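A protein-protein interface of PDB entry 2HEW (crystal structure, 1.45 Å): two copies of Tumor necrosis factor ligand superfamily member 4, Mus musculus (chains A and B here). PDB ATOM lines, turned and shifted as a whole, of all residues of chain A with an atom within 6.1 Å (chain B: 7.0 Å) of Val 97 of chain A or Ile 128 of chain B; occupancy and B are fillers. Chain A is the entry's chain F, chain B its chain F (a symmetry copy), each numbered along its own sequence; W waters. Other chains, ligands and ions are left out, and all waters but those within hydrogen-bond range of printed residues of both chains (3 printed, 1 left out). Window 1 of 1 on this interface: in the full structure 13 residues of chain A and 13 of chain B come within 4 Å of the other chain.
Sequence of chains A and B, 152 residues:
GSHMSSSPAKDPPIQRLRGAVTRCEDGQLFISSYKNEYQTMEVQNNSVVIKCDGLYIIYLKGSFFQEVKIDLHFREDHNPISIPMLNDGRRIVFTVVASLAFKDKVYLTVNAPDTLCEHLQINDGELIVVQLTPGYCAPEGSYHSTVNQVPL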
ATOM      1  N   LEU A  55      -4.480  19.367 -26.384  1.00  0.00           N
ATOM      2  CA  LEU A  55      -4.386  20.240 -25.222  1.00  0.00           C
ATOM      3  C   LEU A  55      -3.811  19.405 -24.091  1.00  0.00           C
ATOM      4  O   LEU A  55      -4.219  18.254 -23.903  1.00  0.00           O
ATOM      5  CB  LEU A  55      -5.743  20.800 -24.821  1.00  0.00           C
ATOM      6  CG  LEU A  55      -6.364  21.757 -25.840  1.00  0.00           C
ATOM      7  CD1 LEU A  55      -7.795  22.089 -25.455  1.00  0.00           C
ATOM      8  CD2 LEU A  55      -5.550  23.026 -25.963  1.00  0.00           C
ATOM      9  N   TYR A  56      -2.811  19.950 -23.408  1.00  0.00           N
ATOM     10  CA  TYR A  56      -2.185  19.292 -22.271  1.00  0.00           C
ATOM     11  C   TYR A  56      -2.192  20.212 -21.056  1.00  0.00           C
ATOM     12  O   TYR A  56      -2.063  21.433 -21.185  1.00  0.00           O
ATOM     13  CB  TYR A  56      -0.722  18.993 -22.561  1.00  0.00           C
ATOM     14  CG  TYR A  56      -0.405  17.869 -23.527  1.00  0.00           C
ATOM     15  CD1 TYR A  56      -0.634  17.997 -24.892  1.00  0.00           C
ATOM     16  CD2 TYR A  56       0.180  16.690 -23.073  1.00  0.00           C
ATOM     17  CE1 TYR A  56      -0.306  16.965 -25.782  1.00  0.00           C
ATOM     18  CE2 TYR A  56       0.533  15.668 -23.952  1.00  0.00           C
ATOM     19  CZ  TYR A  56       0.278  15.799 -25.299  1.00  0.00           C
ATOM     20  OH  TYR A  56       0.636  14.764 -26.136  1.00  0.00           O
ATOM     21  N   ILE A  57      -2.317  19.621 -19.873  1.00  0.00           N
ATOM     22  CA  ILE A  57      -1.888  20.328 -18.664  1.00  0.00           C
ATOM     23  C   ILE A  57      -0.406  20.121 -18.454  1.00  0.00           C
ATOM     24  O   ILE A  57       0.116  19.031 -18.673  1.00  0.00           O
ATOM     25  CB  ILE A  57      -2.570  19.747 -17.419  1.00  0.00           C
ATOM     26  CG1 ILE A  57      -4.050  20.067 -17.427  1.00  0.00           C
ATOM     27  CG2 ILE A  57      -1.902  20.268 -16.125  1.00  0.00           C
ATOM     28  CD1 ILE A  57      -4.825  19.426 -16.295  1.00  0.00           C
ATOM     29  N   ILE A  58       0.261  21.203 -18.058  1.00  0.00           N
ATOM     30  CA  ILE A  58       1.649  21.175 -17.629  1.00  0.00           C
ATOM     31  C   ILE A  58       1.621  21.748 -16.220  1.00  0.00           C
ATOM     32  O   ILE A  58       1.164  22.870 -16.011  1.00  0.00           O
ATOM     33  CB  ILE A  58       2.583  22.011 -18.531  1.00  0.00           C
ATOM     34  CG1 ILE A  58       2.488  21.526 -19.987  1.00  0.00           C
ATOM     35  CG2 ILE A  58       4.032  21.923 -18.030  1.00  0.00           C
ATOM     36  CD1 ILE A  58       3.184  22.426 -20.989  1.00  0.00           C
ATOM     37  N   THR A  95       0.040  25.633 -12.638  1.00  0.00           N
ATOM     38  CA  THR A  95      -0.664  24.893 -13.677  1.00  0.00           C
ATOM     39  C   THR A  95      -0.840  25.749 -14.923  1.00  0.00           C
ATOM     40  O   THR A  95      -1.310  26.894 -14.849  1.00  0.00           O
ATOM     41  CB  THR A  95      -2.050  24.461 -13.164  1.00  0.00           C
ATOM     42  OG1 THR A  95      -1.901  23.785 -11.909  1.00  0.00           O
ATOM     43  CG2 THR A  95      -2.742  23.551 -14.167  1.00  0.00           C
ATOM     44  N   VAL A  96      -0.483  25.161 -16.057  1.00  0.00           N
ATOM     45  CA  VAL A  96      -0.678  25.749 -17.372  1.00  0.00           C
ATOM     46  C   VAL A  96      -1.479  24.753 -18.207  1.00  0.00           C
ATOM     47  O   VAL A  96      -1.359  23.547 -18.019  1.00  0.00           O
ATOM     48  CB  VAL A  96       0.709  26.007 -18.036  1.00  0.00           C
ATOM     49  CG1 VAL A  96       0.597  26.302 -19.523  1.00  0.00           C
ATOM     50  CG2 VAL A  96       1.429  27.144 -17.303  1.00  0.00           C
ATOM     51  N   VAL A  97      -2.318  25.261 -19.102  1.00  0.00           N
ATOM     52  CA  VAL A  97      -2.903  24.456 -20.158  1.00  0.00           C
ATOM     53  C   VAL A  97      -2.378  24.999 -21.475  1.00  0.00           C
ATOM     54  O   VAL A  97      -2.364  26.210 -21.687  1.00  0.00           O
ATOM     55  CB  VAL A  97      -4.438  24.481 -20.139  1.00  0.00           C
ATOM     56  CG1 VAL A  97      -4.993  23.543 -21.218  1.00  0.00           C
ATOM     57  CG2 VAL A  97      -4.951  24.095 -18.753  1.00  0.00           C
ATOM     58  N   ALA A  98      -1.924  24.103 -22.340  1.00  0.00           N
ATOM     59  CA  ALA A  98      -1.286  24.515 -23.578  1.00  0.00           C
ATOM     60  C   ALA A  98      -1.600  23.564 -24.705  1.00  0.00           C
ATOM     61  O   ALA A  98      -1.952  22.409 -24.474  1.00  0.00           O
ATOM     62  CB  ALA A  98       0.211  24.617 -23.391  1.00  0.00           C
ATOM     63  N   SER A  99      -1.456  24.070 -25.923  1.00  0.00           N
ATOM     64  CA  SER A  99      -1.693  23.298 -27.131  1.00  0.00           C
ATOM     65  C   SER A  99      -0.350  22.829 -27.677  1.00  0.00           C
ATOM     66  O   SER A  99       0.424  23.626 -28.191  1.00  0.00           O
ATOM     67  CB  SER A  99      -2.418  24.172 -28.157  1.00  0.00           C
ATOM     68  OG  SER A  99      -2.702  23.469 -29.349  1.00  0.00           O
ATOM     69  N   LEU A 132      -5.133  16.155 -22.454  1.00  0.00           N
ATOM     70  CA  LEU A 132      -6.569  16.286 -22.196  1.00  0.00           C
ATOM     71  C   LEU A 132      -7.446  16.005 -23.404  1.00  0.00           C
ATOM     72  O   LEU A 132      -8.609  15.646 -23.245  1.00  0.00           O
ATOM     73  CB  LEU A 132      -6.896  17.695 -21.717  1.00  0.00           C
ATOM     74  CG  LEU A 132      -6.135  18.179 -20.494  1.00  0.00           C
ATOM     75  CD1 LEU A 132      -6.534  19.597 -20.207  1.00  0.00           C
ATOM     76  CD2 LEU A 132      -6.395  17.292 -19.294  1.00  0.00           C
ATOM     77  N   ARG B  16     -14.015  21.053 -26.443  1.00  0.00           N
ATOM     78  CA  ARG B  16     -12.982  22.031 -26.142  1.00  0.00           C
ATOM     79  C   ARG B  16     -13.020  23.223 -27.061  1.00  0.00           C
ATOM     80  O   ARG B  16     -13.489  23.156 -28.206  1.00  0.00           O
ATOM     81  CB  ARG B  16     -11.570  21.420 -26.147  1.00  0.00           C
ATOM     82  CG  ARG B  16     -11.011  21.036 -27.501  1.00  0.00           C
ATOM     83  CD  ARG B  16     -11.540  19.689 -27.971  1.00  0.00           C
ATOM     84  NE  ARG B  16     -10.589  19.019 -28.849  1.00  0.00           N
ATOM     85  CZ  ARG B  16     -10.738  17.783 -29.311  1.00  0.00           C
ATOM     86  NH1 ARG B  16     -11.783  17.045 -28.970  1.00  0.00           N
ATOM     87  NH2 ARG B  16      -9.814  17.267 -30.100  1.00  0.00           N
ATOM     88  N   LEU B  17     -12.498  24.316 -26.535  1.00  0.00           N
ATOM     89  CA  LEU B  17     -12.303  25.521 -27.296  1.00  0.00           C
ATOM     90  C   LEU B  17     -11.075  26.231 -26.751  1.00  0.00           C
ATOM     91  O   LEU B  17     -10.922  26.359 -25.539  1.00  0.00           O
ATOM     92  CB  LEU B  17     -13.532  26.416 -27.180  1.00  0.00           C
ATOM     93  CG  LEU B  17     -13.394  27.678 -28.040  1.00  0.00           C
ATOM     94  CD1 LEU B  17     -14.561  27.819 -28.985  1.00  0.00           C
ATOM     95  CD2 LEU B  17     -13.148  28.921 -27.194  1.00  0.00           C
ATOM     96  N   ARG B  18     -10.208  26.702 -27.650  1.00  0.00           N
ATOM     97  CA  ARG B  18      -9.109  27.586 -27.261  1.00  0.00           C
ATOM     98  C   ARG B  18      -9.292  28.860 -28.054  1.00  0.00           C
ATOM     99  O   ARG B  18      -9.159  28.852 -29.274  1.00  0.00           O
ATOM    100  CB  ARG B  18      -7.742  26.967 -27.533  1.00  0.00           C
ATOM    101  CG  ARG B  18      -6.568  27.882 -27.135  1.00  0.00           C
ATOM    102  CD  ARG B  18      -5.277  27.098 -26.964  1.00  0.00           C
ATOM    103  NE  ARG B  18      -4.843  26.627 -28.267  1.00  0.00           N
ATOM    104  CZ  ARG B  18      -3.968  27.233 -29.064  1.00  0.00           C
ATOM    105  NH1 ARG B  18      -3.346  28.348 -28.713  1.00  0.00           N
ATOM    106  NH2 ARG B  18      -3.694  26.692 -30.235  1.00  0.00           N
ATOM    107  N   GLY B  19      -9.644  29.936 -27.364  1.00  0.00           N
ATOM    108  CA  GLY B  19      -9.959  31.197 -28.015  1.00  0.00           C
ATOM    109  C   GLY B  19      -8.962  32.286 -27.702  1.00  0.00           C
ATOM    110  O   GLY B  19      -8.346  32.294 -26.641  1.00  0.00           O
ATOM    111  N   VAL B  21      -8.277  35.987 -26.586  1.00  0.00           N
ATOM    112  CA  VAL B  21      -8.940  37.030 -25.816  1.00  0.00           C
ATOM    113  C   VAL B  21      -8.275  38.311 -26.288  1.00  0.00           C
ATOM    114  O   VAL B  21      -7.136  38.587 -25.938  1.00  0.00           O
ATOM    115  CB  VAL B  21      -8.783  36.802 -24.297  1.00  0.00           C
ATOM    116  CG1 VAL B  21      -9.478  37.893 -23.521  1.00  0.00           C
ATOM    117  CG2 VAL B  21      -9.343  35.441 -23.914  1.00  0.00           C
ATOM    118  N   GLU B  37      -6.248  25.570 -33.279  1.00  0.00           N
ATOM    119  CA  GLU B  37      -6.822  24.552 -32.429  1.00  0.00           C
ATOM    120  C   GLU B  37      -8.032  23.975 -33.119  1.00  0.00           C
ATOM    121  O   GLU B  37      -8.804  24.706 -33.736  1.00  0.00           O
ATOM    122  CB  GLU B  37      -7.259  25.145 -31.092  1.00  0.00           C
ATOM    123  CG  GLU B  37      -7.571  24.104 -30.026  1.00  0.00           C
ATOM    124  CD  GLU B  37      -6.330  23.385 -29.560  1.00  0.00           C
ATOM    125  OE1 GLU B  37      -5.282  24.055 -29.417  1.00  0.00           O
ATOM    126  OE2 GLU B  37      -6.386  22.161 -29.355  1.00  0.00           O
ATOM    127  N   ILE B  57     -12.227  22.190 -17.259  1.00  0.00           N
ATOM    128  CA  ILE B  57     -11.264  23.234 -16.900  1.00  0.00           C
ATOM    129  C   ILE B  57     -11.537  24.478 -17.713  1.00  0.00           C
ATOM    130  O   ILE B  57     -11.855  24.401 -18.898  1.00  0.00           O
ATOM    131  CB  ILE B  57      -9.834  22.808 -17.261  1.00  0.00           C
ATOM    132  CG1 ILE B  57      -9.377  21.677 -16.363  1.00  0.00           C
ATOM    133  CG2 ILE B  57      -8.860  24.006 -17.176  1.00  0.00           C
ATOM    134  CD1 ILE B  57      -8.022  21.110 -16.730  1.00  0.00           C
ATOM    135  N   ILE B  58     -11.440  25.622 -17.040  1.00  0.00           N
ATOM    136  CA  ILE B  58     -11.486  26.930 -17.672  1.00  0.00           C
ATOM    137  C   ILE B  58     -10.178  27.592 -17.266  1.00  0.00           C
ATOM    138  O   ILE B  58      -9.892  27.735 -16.079  1.00  0.00           O
ATOM    139  CB  ILE B  58     -12.687  27.786 -17.214  1.00  0.00           C
ATOM    140  CG1 ILE B  58     -14.004  27.040 -17.486  1.00  0.00           C
ATOM    141  CG2 ILE B  58     -12.682  29.144 -17.932  1.00  0.00           C
ATOM    142  CD1 ILE B  58     -15.225  27.689 -16.863  1.00  0.00           C
ATOM    143  N   TYR B  59      -9.394  27.979 -18.264  1.00  0.00           N
ATOM    144  CA  TYR B  59      -8.048  28.490 -18.078  1.00  0.00           C
ATOM    145  C   TYR B  59      -7.925  29.797 -18.837  1.00  0.00           C
ATOM    146  O   TYR B  59      -8.303  29.876 -20.006  1.00  0.00           O
ATOM    147  CB  TYR B  59      -7.053  27.477 -18.606  1.00  0.00           C
ATOM    148  CG  TYR B  59      -5.641  27.952 -18.810  1.00  0.00           C
ATOM    149  CD1 TYR B  59      -4.729  27.944 -17.770  1.00  0.00           C
ATOM    150  CD2 TYR B  59      -5.205  28.364 -20.062  1.00  0.00           C
ATOM    151  CE1 TYR B  59      -3.416  28.358 -17.959  1.00  0.00           C
ATOM    152  CE2 TYR B  59      -3.901  28.762 -20.268  1.00  0.00           C
ATOM    153  CZ  TYR B  59      -3.002  28.747 -19.210  1.00  0.00           C
ATOM    154  OH  TYR B  59      -1.706  29.139 -19.426  1.00  0.00           O
ATOM    155  N   LEU B  60      -7.407  30.818 -18.162  1.00  0.00           N
ATOM    156  CA  LEU B  60      -7.193  32.122 -18.780  1.00  0.00           C
ATOM    157  C   LEU B  60      -5.742  32.507 -18.594  1.00  0.00           C
ATOM    158  O   LEU B  60      -5.211  32.413 -17.491  1.00  0.00           O
ATOM    159  CB  LEU B  60      -8.081  33.193 -18.138  1.00  0.00           C
ATOM    160  CG  LEU B  60      -7.947  34.612 -18.716  1.00  0.00           C
ATOM    161  CD1 LEU B  60      -8.415  34.679 -20.155  1.00  0.00           C
ATOM    162  CD2 LEU B  60      -8.718  35.612 -17.876  1.00  0.00           C
ATOM    163  N   LYS B  61      -5.125  32.952 -19.682  1.00  0.00           N
ATOM    164  CA  LYS B  61      -3.762  33.467 -19.665  1.00  0.00           C
ATOM    165  C   LYS B  61      -3.729  34.763 -20.457  1.00  0.00           C
ATOM    166  O   LYS B  61      -4.416  34.895 -21.471  1.00  0.00           O
ATOM    167  CB  LYS B  61      -2.808  32.437 -20.297  1.00  0.00           C
ATOM    168  CG  LYS B  61      -1.437  32.970 -20.718  1.00  0.00           C
ATOM    169  CD  LYS B  61      -0.580  31.878 -21.336  1.00  0.00           C
ATOM    170  CE  LYS B  61       0.759  32.423 -21.810  1.00  0.00           C
ATOM    171  NZ  LYS B  61       1.418  31.523 -22.803  1.00  0.00           N
ATOM    172  N   VAL B  93      -2.509  33.999 -15.179  1.00  0.00           N
ATOM    173  CA  VAL B  93      -2.439  32.584 -15.559  1.00  0.00           C
ATOM    174  C   VAL B  93      -3.265  31.851 -14.504  1.00  0.00           C
ATOM    175  O   VAL B  93      -2.774  31.577 -13.404  1.00  0.00           O
ATOM    176  CB  VAL B  93      -0.989  32.015 -15.548  1.00  0.00           C
ATOM    177  CG1 VAL B  93      -0.989  30.566 -16.040  1.00  0.00           C
ATOM    178  CG2 VAL B  93      -0.043  32.857 -16.387  1.00  0.00           C
ATOM    179  N   PHE B  94      -4.518  31.553 -14.837  1.00  0.00           N
ATOM    180  CA  PHE B  94      -5.515  31.172 -13.835  1.00  0.00           C
ATOM    181  C   PHE B  94      -6.310  29.967 -14.305  1.00  0.00           C
ATOM    182  O   PHE B  94      -6.754  29.925 -15.448  1.00  0.00           O
ATOM    183  CB  PHE B  94      -6.464  32.345 -13.599  1.00  0.00           C
ATOM    184  CG  PHE B  94      -7.359  32.173 -12.408  1.00  0.00           C
ATOM    185  CD1 PHE B  94      -6.829  32.051 -11.139  1.00  0.00           C
ATOM    186  CD2 PHE B  94      -8.733  32.171 -12.560  1.00  0.00           C
ATOM    187  CE1 PHE B  94      -7.666  31.896 -10.025  1.00  0.00           C
ATOM    188  CE2 PHE B  94      -9.574  32.029 -11.459  1.00  0.00           C
ATOM    189  CZ  PHE B  94      -9.038  31.895 -10.200  1.00  0.00           C
ATOM    190  N   THR B  95      -6.491  28.999 -13.412  1.00  0.00           N
ATOM    191  CA  THR B  95      -7.203  27.760 -13.702  1.00  0.00           C
ATOM    192  C   THR B  95      -8.368  27.570 -12.742  1.00  0.00           C
ATOM    193  O   THR B  95      -8.207  27.668 -11.516  1.00  0.00           O
ATOM    194  CB  THR B  95      -6.244  26.563 -13.573  1.00  0.00           C
ATOM    195  OG1 THR B  95      -5.071  26.808 -14.360  1.00  0.00           O
ATOM    196  CG2 THR B  95      -6.915  25.277 -14.027  1.00  0.00           C
ATOM    197  N   VAL B  96      -9.523  27.269 -13.320  1.00  0.00           N
ATOM    198  CA  VAL B  96     -10.732  26.929 -12.589  1.00  0.00           C
ATOM    199  C   VAL B  96     -11.205  25.566 -13.091  1.00  0.00           C
ATOM    200  O   VAL B  96     -11.002  25.227 -14.252  1.00  0.00           O
ATOM    201  CB  VAL B  96     -11.825  28.006 -12.863  1.00  0.00           C
ATOM    202  CG1 VAL B  96     -13.208  27.560 -12.417  1.00  0.00           C
ATOM    203  CG2 VAL B  96     -11.429  29.325 -12.191  1.00  0.00           C
ATOM    204  N   GLU B 126      -5.493  34.216 -24.031  1.00  0.00           N
ATOM    205  CA  GLU B 126      -6.268  33.073 -24.469  1.00  0.00           C
ATOM    206  C   GLU B 126      -7.101  32.471 -23.358  1.00  0.00           C
ATOM    207  O   GLU B 126      -6.738  32.518 -22.180  1.00  0.00           O
ATOM    208  CB  GLU B 126      -5.399  32.009 -25.152  1.00  0.00           C
ATOM    209  CG  GLU B 126      -4.448  31.294 -24.264  1.00  0.00           C
ATOM    210  CD  GLU B 126      -3.680  30.176 -24.977  1.00  0.00           C
ATOM    211  OE1 GLU B 126      -3.756  30.054 -26.222  1.00  0.00           O
ATOM    212  OE2 GLU B 126      -2.990  29.424 -24.268  1.00  0.00           O
ATOM    213  N   LEU B 127      -8.245  31.936 -23.762  1.00  0.00           N
ATOM    214  CA  LEU B 127      -9.170  31.251 -22.888  1.00  0.00           C
ATOM    215  C   LEU B 127      -9.282  29.828 -23.410  1.00  0.00           C
ATOM    216  O   LEU B 127      -9.551  29.624 -24.596  1.00  0.00           O
ATOM    217  CB  LEU B 127     -10.539  31.936 -22.931  1.00  0.00           C
ATOM    218  CG  LEU B 127     -11.628  31.288 -22.066  1.00  0.00           C
ATOM    219  CD1 LEU B 127     -11.357  31.539 -20.609  1.00  0.00           C
ATOM    220  CD2 LEU B 127     -13.002  31.824 -22.454  1.00  0.00           C
ATOM    221  N   ILE B 128      -9.068  28.857 -22.530  1.00  0.00           N
ATOM    222  CA  ILE B 128      -9.220  27.450 -22.866  1.00  0.00           C
ATOM    223  C   ILE B 128     -10.315  26.868 -22.000  1.00  0.00           C
ATOM    224  O   ILE B 128     -10.276  26.990 -20.783  1.00  0.00           O
ATOM    225  CB  ILE B 128      -7.917  26.664 -22.669  1.00  0.00           C
ATOM    226  CG1 ILE B 128      -6.832  27.242 -23.590  1.00  0.00           C
ATOM    227  CG2 ILE B 128      -8.149  25.197 -22.980  1.00  0.00           C
ATOM    228  CD1 ILE B 128      -5.426  26.634 -23.420  1.00  0.00           C
ATOM    229  N   VAL B 129     -11.308  26.270 -22.651  1.00  0.00           N
ATOM    230  CA  VAL B 129     -12.383  25.559 -21.983  1.00  0.00           C
ATOM    231  C   VAL B 129     -12.318  24.114 -22.465  1.00  0.00           C
ATOM    232  O   VAL B 129     -12.411  23.864 -23.663  1.00  0.00           O
ATOM    233  CB  VAL B 129     -13.748  26.165 -22.328  1.00  0.00           C
ATOM    234  CG1 VAL B 129     -14.849  25.439 -21.589  1.00  0.00           C
ATOM    235  CG2 VAL B 129     -13.771  27.653 -21.984  1.00  0.00           C
ATOM    236  N   VAL B 130     -12.115  23.171 -21.551  1.00  0.00           N
ATOM    237  CA  VAL B 130     -11.925  21.777 -21.943  1.00  0.00           C
ATOM    238  C   VAL B 130     -12.640  20.812 -21.007  1.00  0.00           C
ATOM    239  O   VAL B 130     -12.486  20.869 -19.793  1.00  0.00           O
ATOM    240  CB  VAL B 130     -10.428  21.432 -22.131  1.00  0.00           C
ATOM    241  CG1 VAL B 130      -9.623  21.785 -20.941  1.00  0.00           C
ATOM    242  CG2 VAL B 130     -10.236  19.980 -22.536  1.00  0.00           C
HETATM  243  O   HOH W   1      -1.265  28.641 -22.104  1.00  0.00           O
HETATM  244  O   HOH W   2      -3.091  28.430 -13.421  1.00  0.00           O
HETATM  245  O   HOH W   3      -1.402  24.514 -31.528  1.00  0.00           O
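Among the printed residues, merely in contact across the chains: Leu 55 of chain A with Arg 16 of chain B (3.9 Å), Leu 55 of chain A with Glu 37 of chain B (3.5 Å), Leu 55 of chain A with Ile 128 of chain B (3.99 Å), Ile 57 of chain A with Ile 57 of chain B (3.6 Å), Thr 95 of chain A with Val 93 of chain B (3.9 Å), Thr 95 of chain A with Thr 95 of chain B (3.8 Å), Val 96 of chain A with Tyr 59 of chain B (3.7 Å), Val 97 of chain A with Tyr 59 of chain B (3.3 Å), Val 97 of chain A with Ile 128 of chain B (3.5 Å) and Leu 132 of chain A with Val 130 of chain B (3.9 Å).
The backbone carbonyl oxygen (O) of Leu 55 of chain A lies within hydrogen-bond range of the backbone NH (N) of Leu 132 of chain A, 2.7 Å away. The backbone carbonyl oxygen (O) of Ile 58 of chain A lies within hydrogen-bond range of the backbone NH (N) of Val 96 of chain A, 2.8 Å away. NE of Arg 18 of chain B lies within salt-bridge range of OE1 of Glu 37 of chain B, 2.9 Å away. The guanidinium group (NH1) of Arg 18 of chain B is in salt-bridge range of the side-chain carboxylate (OE1) of Glu 126 of chain B (3.0 Å). N of Ile 57 of chain B sits at hydrogen-bond distance from O of Val 130 of chain B (2.9 Å). O of Tyr 59 of chain B sits at hydrogen-bond distance from N of Ile 128 of chain B (2.8 Å).
Ile 57 of chain B touches its own counterpart, Ile 57 of chain A. Thr 95 of chain B touches its own counterpart, Thr 95 of chain A.
Hydrophobic or aromatic side chains of chain B within 4 Å of the printed part of chain A: Ile 57, Tyr 59, Val 93, Ile 128 and Val 130. Of the 10 printed residues of chain A, 7 touch a printed residue of chain B. Among the printed residues, 12 pairs touch across the chains. Among the printed residues, no Asp or Glu carboxylate lies within 4 Å of a Lys or Arg side-chain nitrogen of the other chain.
Of the printed residues of chain B, Thr 95 of chain A touches Val 93 (3.9 Å) and Thr 95 (3.8 Å). Val 97 of chain A touches just these residues of chain B: Tyr 59 and Ile 128. Printed residues of chain B within 4 Å of Leu 132 of chain A: Val 130 (3.9 Å). Val 21 of chain B touches none of the printed residues of chain A. Of the printed residues of chain A, Ile 57 of chain B touches Ile 57 (3.6 Å). Of the printed residues of chain A, Thr 95 of chain B touches Thr 95. Printed residues of chain A within 4 Å of Ile 128 of chain B: Leu 55 (3.99 Å) and Val 97 (3.5 Å). Of the printed residues of chain A, Val 130 of chain B touches Leu 132. The nearest printed residue of chain A that does not touch Ile 128 of chain B is Ala 98 of chain A (4.5 Å). The nearest printed residue of chain A that does not touch Val 130 of chain B is Leu 55 of chain A (4.3 Å).
Water W1 lies within hydrogen-bond range of the backbone carbonyl oxygen of Val 97 of chain A, the side-chain hydroxyl of Tyr 59 of chain B and the side-chain carboxylate of Glu 126 of chain B. Water W2 lies within hydrogen-bond range of the side-chain hydroxyl of Thr 95 of chain B (2.7 Å), the backbone carbonyl oxygen of Thr 95 of chain A (2.8 Å) and the backbone carbonyl oxygen of Val 93 of chain B (3.2 Å). Water W3 bridges OG of Ser 99 of chain A (2.7 Å) and NH2 of Arg 18 of chain B (3.4 Å).
The guanidinium group (NH2) of Arg 18 of chain B lies within hydrogen-bond range of the side-chain hydroxyl (OG) of Ser 99 of chain A. OE1 of Glu 37 of chain B is in hydrogen-bond range of OG of Ser 99 of chain A, 2.6 Å away.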
